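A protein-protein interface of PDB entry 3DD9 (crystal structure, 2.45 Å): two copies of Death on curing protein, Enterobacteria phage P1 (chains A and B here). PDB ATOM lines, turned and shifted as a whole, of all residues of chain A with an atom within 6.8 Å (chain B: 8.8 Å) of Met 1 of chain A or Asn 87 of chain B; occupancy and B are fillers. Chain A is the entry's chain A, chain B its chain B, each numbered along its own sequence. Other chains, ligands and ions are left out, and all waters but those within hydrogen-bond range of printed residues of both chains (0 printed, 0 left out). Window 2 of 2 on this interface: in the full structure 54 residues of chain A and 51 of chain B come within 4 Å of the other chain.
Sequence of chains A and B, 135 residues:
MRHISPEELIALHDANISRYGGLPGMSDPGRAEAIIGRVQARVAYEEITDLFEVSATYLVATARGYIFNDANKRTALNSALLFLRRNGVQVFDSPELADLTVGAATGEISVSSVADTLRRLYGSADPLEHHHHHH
No position is printed for both chains.
ND2 of Asn 87 of chain B lies within hydrogen-bond range of O of Phe 83 of chain B, 2.7 Å away.
N of Val 89 of chain B sits at hydrogen-bond distance from O of Leu 84 of chain B (3.1 Å).
Printed residues of chain B within 4 Å of Met 1 of chain A: Phe 83 (3.98 Å) and Asn 87 (3.2 Å).
Printed residues of chain B within 4 Å of His 3 of chain A: Arg 86.
Printed residues of chain B within 4 Å of Val 54 of chain A: Phe 83.
Printed residues of chain A within 4 Å of Leu 84 of chain B: Leu 51.
Hydrophobic or aromatic side chains of chain B that line the printed part of chain A: Phe 83 and Leu 84.
Of the 10 printed residues of chain A, 6 touch a printed residue of chain B.
Hydrophobic or aromatic side chains of chain A that line the printed part of chain B: Met 1, Leu 51, Val 54 and Tyr 58.
Among the printed residues, no Asp or Glu carboxylate lies within 4 Å of a Lys or Arg side-chain nitrogen of the other chain.
NH2 of Arg 2 of chain A sits close to NE of Arg 86 of chain B (3.3 Å).
The backbone NH (N) of Arg 2 of chain A is in hydrogen-bond range of the side-chain amide oxygen (OD1) of Asn 87 of chain B (2.5 Å).
The guanidinium group (NH2) of Arg 86 of chain B lies within hydrogen-bond range of the backbone carbonyl oxygen (O) of His 3 of chain A (3.0 Å).
Among the printed residues, merely in contact across the chains: Met 1 of chain A with Asn 87 of chain B (3.2 Å), Leu 51 of chain A with Phe 83 of chain B (3.2 Å), Arg 2 of chain A with Phe 83 of chain B (3.3 Å), Val 54 of chain A with Phe 83 of chain B (3.5 Å), Tyr 58 of chain A with Phe 83 of chain B (3.7 Å), Leu 51 of chain A with Asn 87 of chain B (3.7 Å), Tyr 58 of chain A with Ser 79 of chain B (3.7 Å), Leu 51 of chain A with Leu 84 of chain B (3.9 Å) and Met 1 of chain A with Phe 83 of chain B (3.98 Å).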
ATOM      1  N   MET A   1     -16.466   5.716 -15.822  1.00  0.00           N
ATOM      2  CA  MET A   1     -15.367   6.616 -16.298  1.00  0.00           C
ATOM      3  C   MET A   1     -14.024   6.176 -15.734  1.00  0.00           C
ATOM      4  O   MET A   1     -13.965   5.478 -14.725  1.00  0.00           O
ATOM      5  CB  MET A   1     -15.652   8.088 -15.963  1.00  0.00           C
ATOM      6  CG  MET A   1     -15.987   8.346 -14.508  1.00  0.00           C
ATOM      7  SD  MET A   1     -16.140  10.092 -14.106  1.00  0.00           S
ATOM      8  CE  MET A   1     -17.441  10.601 -15.259  1.00  0.00           C
ATOM      9  N   ARG A   2     -12.954   6.569 -16.421  1.00  0.00           N
ATOM     10  CA  ARG A   2     -11.606   6.215 -16.039  1.00  0.00           C
ATOM     11  C   ARG A   2     -10.898   7.398 -15.376  1.00  0.00           C
ATOM     12  O   ARG A   2     -10.735   8.459 -15.990  1.00  0.00           O
ATOM     13  CB  ARG A   2     -10.826   5.806 -17.289  1.00  0.00           C
ATOM     14  CG  ARG A   2     -11.210   4.461 -17.868  1.00  0.00           C
ATOM     15  CD  ARG A   2     -10.115   3.426 -17.599  1.00  0.00           C
ATOM     16  NE  ARG A   2      -9.098   3.455 -18.657  1.00  0.00           N
ATOM     17  CZ  ARG A   2      -7.792   3.677 -18.471  1.00  0.00           C
ATOM     18  NH1 ARG A   2      -6.999   3.663 -19.527  1.00  0.00           N
ATOM     19  NH2 ARG A   2      -7.270   3.895 -17.253  1.00  0.00           N
ATOM     20  N   HIS A   3     -10.438   7.191 -14.145  1.00  0.00           N
ATOM     21  CA  HIS A   3      -9.745   8.224 -13.396  1.00  0.00           C
ATOM     22  C   HIS A   3      -8.242   8.203 -13.554  1.00  0.00           C
ATOM     23  O   HIS A   3      -7.690   7.326 -14.175  1.00  0.00           O
ATOM     24  CB  HIS A   3     -10.127   8.157 -11.926  1.00  0.00           C
ATOM     25  CG  HIS A   3     -11.474   8.731 -11.658  1.00  0.00           C
ATOM     26  ND1 HIS A   3     -11.684  10.085 -11.525  1.00  0.00           N
ATOM     27  CD2 HIS A   3     -12.689   8.147 -11.541  1.00  0.00           C
ATOM     28  CE1 HIS A   3     -12.970  10.309 -11.309  1.00  0.00           C
ATOM     29  NE2 HIS A   3     -13.600   9.152 -11.311  1.00  0.00           N
ATOM     30  N   VAL A  43     -16.571  13.647  -6.846  1.00  0.00           N
ATOM     31  CA  VAL A  43     -17.279  13.070  -7.974  1.00  0.00           C
ATOM     32  C   VAL A  43     -18.302  12.023  -7.507  1.00  0.00           C
ATOM     33  O   VAL A  43     -19.426  11.985  -7.990  1.00  0.00           O
ATOM     34  CB  VAL A  43     -16.303  12.555  -9.064  1.00  0.00           C
ATOM     35  CG1 VAL A  43     -17.004  11.635 -10.031  1.00  0.00           C
ATOM     36  CG2 VAL A  43     -15.714  13.742  -9.806  1.00  0.00           C
ATOM     37  N   ILE A  48     -21.221  13.601  -9.708  1.00  0.00           N
ATOM     38  CA  ILE A  48     -20.820  14.311 -10.903  1.00  0.00           C
ATOM     39  C   ILE A  48     -20.612  13.293 -11.998  1.00  0.00           C
ATOM     40  O   ILE A  48     -19.705  12.452 -11.923  1.00  0.00           O
ATOM     41  CB  ILE A  48     -19.584  15.208 -10.725  1.00  0.00           C
ATOM     42  CG1 ILE A  48     -19.827  16.261  -9.623  1.00  0.00           C
ATOM     43  CG2 ILE A  48     -19.254  15.864 -12.060  1.00  0.00           C
ATOM     44  CD1 ILE A  48     -18.556  17.031  -9.187  1.00  0.00           C
ATOM     45  N   THR A  49     -21.465  13.400 -13.013  1.00  0.00           N
ATOM     46  CA  THR A  49     -21.621  12.381 -14.040  1.00  0.00           C
ATOM     47  C   THR A  49     -21.106  12.786 -15.429  1.00  0.00           C
ATOM     48  O   THR A  49     -20.768  11.915 -16.239  1.00  0.00           O
ATOM     49  CB  THR A  49     -23.096  11.931 -14.157  1.00  0.00           C
ATOM     50  OG1 THR A  49     -23.409  11.728 -15.536  1.00  0.00           O
ATOM     51  CG2 THR A  49     -24.068  12.996 -13.607  1.00  0.00           C
ATOM     52  N   ASP A  50     -21.047  14.075 -15.744  1.00  0.00           N
ATOM     53  CA  ASP A  50     -20.525  14.358 -17.061  1.00  0.00           C
ATOM     54  C   ASP A  50     -19.046  14.710 -17.098  1.00  0.00           C
ATOM     55  O   ASP A  50     -18.509  15.367 -16.187  1.00  0.00           O
ATOM     56  CB  ASP A  50     -21.403  15.293 -17.904  1.00  0.00           C
ATOM     57  CG  ASP A  50     -21.115  16.723 -17.660  1.00  0.00           C
ATOM     58  OD1 ASP A  50     -20.593  17.404 -18.595  1.00  0.00           O
ATOM     59  OD2 ASP A  50     -21.407  17.140 -16.506  1.00  0.00           O
ATOM     60  N   LEU A  51     -18.423  14.251 -18.180  1.00  0.00           N
ATOM     61  CA  LEU A  51     -16.986  14.212 -18.346  1.00  0.00           C
ATOM     62  C   LEU A  51     -16.295  15.561 -18.191  1.00  0.00           C
ATOM     63  O   LEU A  51     -15.250  15.656 -17.541  1.00  0.00           O
ATOM     64  CB  LEU A  51     -16.649  13.575 -19.701  1.00  0.00           C
ATOM     65  CG  LEU A  51     -16.924  12.075 -19.674  1.00  0.00           C
ATOM     66  CD1 LEU A  51     -16.604  11.442 -21.033  1.00  0.00           C
ATOM     67  CD2 LEU A  51     -16.103  11.434 -18.567  1.00  0.00           C
ATOM     68  N   VAL A  54     -16.325  16.711 -14.667  1.00  0.00           N
ATOM     69  CA  VAL A  54     -15.309  16.014 -13.907  1.00  0.00           C
ATOM     70  C   VAL A  54     -13.944  16.555 -14.299  1.00  0.00           C
ATOM     71  O   VAL A  54     -13.123  16.820 -13.423  1.00  0.00           O
ATOM     72  CB  VAL A  54     -15.390  14.473 -14.079  1.00  0.00           C
ATOM     73  CG1 VAL A  54     -14.334  13.783 -13.216  1.00  0.00           C
ATOM     74  CG2 VAL A  54     -16.769  13.991 -13.714  1.00  0.00           C
ATOM     75  N   TYR A  58     -10.914  18.195 -11.892  1.00  0.00           N
ATOM     76  CA  TYR A  58      -9.483  17.940 -11.869  1.00  0.00           C
ATOM     77  C   TYR A  58      -8.659  19.212 -12.012  1.00  0.00           C
ATOM     78  O   TYR A  58      -7.658  19.377 -11.309  1.00  0.00           O
ATOM     79  CB  TYR A  58      -9.089  16.987 -12.970  1.00  0.00           C
ATOM     80  CG  TYR A  58      -9.305  15.564 -12.627  1.00  0.00           C
ATOM     81  CD1 TYR A  58      -8.316  14.839 -11.955  1.00  0.00           C
ATOM     82  CD2 TYR A  58     -10.516  14.928 -12.939  1.00  0.00           C
ATOM     83  CE1 TYR A  58      -8.504  13.512 -11.634  1.00  0.00           C
ATOM     84  CE2 TYR A  58     -10.708  13.598 -12.628  1.00  0.00           C
ATOM     85  CZ  TYR A  58      -9.694  12.898 -11.983  1.00  0.00           C
ATOM     86  OH  TYR A  58      -9.906  11.593 -11.624  1.00  0.00           O
ATOM     87  N   SER B  79      -3.666  17.281 -16.164  1.00  0.00           N
ATOM     88  CA  SER B  79      -4.554  16.343 -15.500  1.00  0.00           C
ATOM     89  C   SER B  79      -5.964  16.448 -16.073  1.00  0.00           C
ATOM     90  O   SER B  79      -6.588  15.422 -16.321  1.00  0.00           O
ATOM     91  CB  SER B  79      -4.528  16.533 -13.988  1.00  0.00           C
ATOM     92  OG  SER B  79      -5.202  17.735 -13.576  1.00  0.00           O
ATOM     93  N   ALA B  80      -6.460  17.674 -16.323  1.00  0.00           N
ATOM     94  CA  ALA B  80      -7.822  17.831 -16.850  1.00  0.00           C
ATOM     95  C   ALA B  80      -7.901  17.221 -18.263  1.00  0.00           C
ATOM     96  O   ALA B  80      -8.891  16.609 -18.650  1.00  0.00           O
ATOM     97  CB  ALA B  80      -8.223  19.348 -16.889  1.00  0.00           C
ATOM     98  N   LEU B  81      -6.844  17.418 -19.040  1.00  0.00           N
ATOM     99  CA  LEU B  81      -6.818  16.975 -20.415  1.00  0.00           C
ATOM    100  C   LEU B  81      -6.517  15.468 -20.547  1.00  0.00           C
ATOM    101  O   LEU B  81      -7.077  14.797 -21.448  1.00  0.00           O
ATOM    102  CB  LEU B  81      -5.790  17.810 -21.176  1.00  0.00           C
ATOM    103  CG  LEU B  81      -6.309  19.028 -21.955  1.00  0.00           C
ATOM    104  CD1 LEU B  81      -7.671  19.522 -21.470  1.00  0.00           C
ATOM    105  CD2 LEU B  81      -5.266  20.132 -21.957  1.00  0.00           C
ATOM    106  N   LEU B  82      -5.647  14.933 -19.684  1.00  0.00           N
ATOM    107  CA  LEU B  82      -5.432  13.497 -19.660  1.00  0.00           C
ATOM    108  C   LEU B  82      -6.736  12.749 -19.309  1.00  0.00           C
ATOM    109  O   LEU B  82      -7.063  11.735 -19.909  1.00  0.00           O
ATOM    110  CB  LEU B  82      -4.303  13.108 -18.729  1.00  0.00           C
ATOM    111  CG  LEU B  82      -3.938  11.624 -18.538  1.00  0.00           C
ATOM    112  CD1 LEU B  82      -3.511  10.913 -19.816  1.00  0.00           C
ATOM    113  CD2 LEU B  82      -2.852  11.487 -17.471  1.00  0.00           C
ATOM    114  N   PHE B  83      -7.508  13.281 -18.375  1.00  0.00           N
ATOM    115  CA  PHE B  83      -8.746  12.605 -17.988  1.00  0.00           C
ATOM    116  C   PHE B  83      -9.755  12.580 -19.139  1.00  0.00           C
ATOM    117  O   PHE B  83     -10.486  11.582 -19.305  1.00  0.00           O
ATOM    118  CB  PHE B  83      -9.362  13.244 -16.752  1.00  0.00           C
ATOM    119  CG  PHE B  83     -10.781  12.874 -16.549  1.00  0.00           C
ATOM    120  CD1 PHE B  83     -11.112  11.781 -15.806  1.00  0.00           C
ATOM    121  CD2 PHE B  83     -11.799  13.644 -17.118  1.00  0.00           C
ATOM    122  CE1 PHE B  83     -12.436  11.401 -15.626  1.00  0.00           C
ATOM    123  CE2 PHE B  83     -13.135  13.282 -16.954  1.00  0.00           C
ATOM    124  CZ  PHE B  83     -13.455  12.147 -16.201  1.00  0.00           C
ATOM    125  N   LEU B  84      -9.826  13.668 -19.907  1.00  0.00           N
ATOM    126  CA  LEU B  84     -10.662  13.680 -21.096  1.00  0.00           C
ATOM    127  C   LEU B  84     -10.168  12.677 -22.140  1.00  0.00           C
ATOM    128  O   LEU B  84     -10.958  11.869 -22.618  1.00  0.00           O
ATOM    129  CB  LEU B  84     -10.726  15.066 -21.721  1.00  0.00           C
ATOM    130  CG  LEU B  84     -11.497  16.151 -20.971  1.00  0.00           C
ATOM    131  CD1 LEU B  84     -11.367  17.467 -21.726  1.00  0.00           C
ATOM    132  CD2 LEU B  84     -12.991  15.792 -20.660  1.00  0.00           C
ATOM    133  N   ARG B  85      -8.874  12.713 -22.489  1.00  0.00           N
ATOM    134  CA  ARG B  85      -8.313  11.708 -23.391  1.00  0.00           C
ATOM    135  C   ARG B  85      -8.630  10.290 -22.918  1.00  0.00           C
ATOM    136  O   ARG B  85      -9.171   9.508 -23.683  1.00  0.00           O
ATOM    137  CB  ARG B  85      -6.803  11.888 -23.632  1.00  0.00           C
ATOM    138  N   ARG B  86      -8.322   9.973 -21.663  1.00  0.00           N
ATOM    139  CA  ARG B  86      -8.664   8.663 -21.079  1.00  0.00           C
ATOM    140  C   ARG B  86     -10.109   8.223 -21.307  1.00  0.00           C
ATOM    141  O   ARG B  86     -10.388   7.039 -21.367  1.00  0.00           O
ATOM    142  CB  ARG B  86      -8.448   8.685 -19.571  1.00  0.00           C
ATOM    143  CG  ARG B  86      -7.055   8.443 -19.169  1.00  0.00           C
ATOM    144  CD  ARG B  86      -6.898   7.071 -18.629  1.00  0.00           C
ATOM    145  NE  ARG B  86      -6.491   7.096 -17.224  1.00  0.00           N
ATOM    146  CZ  ARG B  86      -5.229   7.115 -16.801  1.00  0.00           C
ATOM    147  NH1 ARG B  86      -4.221   7.156 -17.666  1.00  0.00           N
ATOM    148  NH2 ARG B  86      -4.986   7.107 -15.498  1.00  0.00           N
ATOM    149  N   ASN B  87     -11.030   9.172 -21.398  1.00  0.00           N
ATOM    150  CA  ASN B  87     -12.426   8.805 -21.513  1.00  0.00           C
ATOM    151  C   ASN B  87     -13.056   9.073 -22.895  1.00  0.00           C
ATOM    152  O   ASN B  87     -14.254   9.349 -23.005  1.00  0.00           O
ATOM    153  CB  ASN B  87     -13.222   9.413 -20.358  1.00  0.00           C
ATOM    154  CG  ASN B  87     -12.816   8.836 -19.017  1.00  0.00           C
ATOM    155  OD1 ASN B  87     -13.444   7.893 -18.521  1.00  0.00           O
ATOM    156  ND2 ASN B  87     -11.750   9.394 -18.416  1.00  0.00           N
ATOM    157  N   GLY B  88     -12.247   8.951 -23.948  1.00  0.00           N
ATOM    158  CA  GLY B  88     -12.746   8.976 -25.327  1.00  0.00           C
ATOM    159  C   GLY B  88     -12.921  10.355 -25.947  1.00  0.00           C
ATOM    160  O   GLY B  88     -13.498  10.487 -27.034  1.00  0.00           O
ATOM    161  N   VAL B  89     -12.441  11.396 -25.276  1.00  0.00           N
ATOM    162  CA  VAL B  89     -12.560  12.752 -25.837  1.00  0.00           C
ATOM    163  C   VAL B  89     -11.251  13.204 -26.458  1.00  0.00           C
ATOM    164  O   VAL B  89     -10.203  13.223 -25.809  1.00  0.00           O
ATOM    165  CB  VAL B  89     -13.080  13.809 -24.807  1.00  0.00           C
ATOM    166  CG1 VAL B  89     -13.033  15.263 -25.402  1.00  0.00           C
ATOM    167  CG2 VAL B  89     -14.488  13.448 -24.350  1.00  0.00           C
ATOM    168  N   GLN B  90     -11.322  13.558 -27.731  1.00  0.00           N
ATOM    169  CA  GLN B  90     -10.149  14.071 -28.413  1.00  0.00           C
ATOM    170  C   GLN B  90      -9.860  15.511 -27.984  1.00  0.00           C
ATOM    171  O   GLN B  90     -10.763  16.338 -27.883  1.00  0.00           O
ATOM    172  CB  GLN B  90     -10.285  13.963 -29.928  1.00  0.00           C
ATOM    173  CG  GLN B  90      -8.933  14.040 -30.604  1.00  0.00           C
ATOM    174  CD  GLN B  90      -8.009  12.913 -30.126  1.00  0.00           C
ATOM    175  OE1 GLN B  90      -8.132  11.767 -30.588  1.00  0.00           O
ATOM    176  NE2 GLN B  90      -7.100  13.229 -29.176  1.00  0.00           N
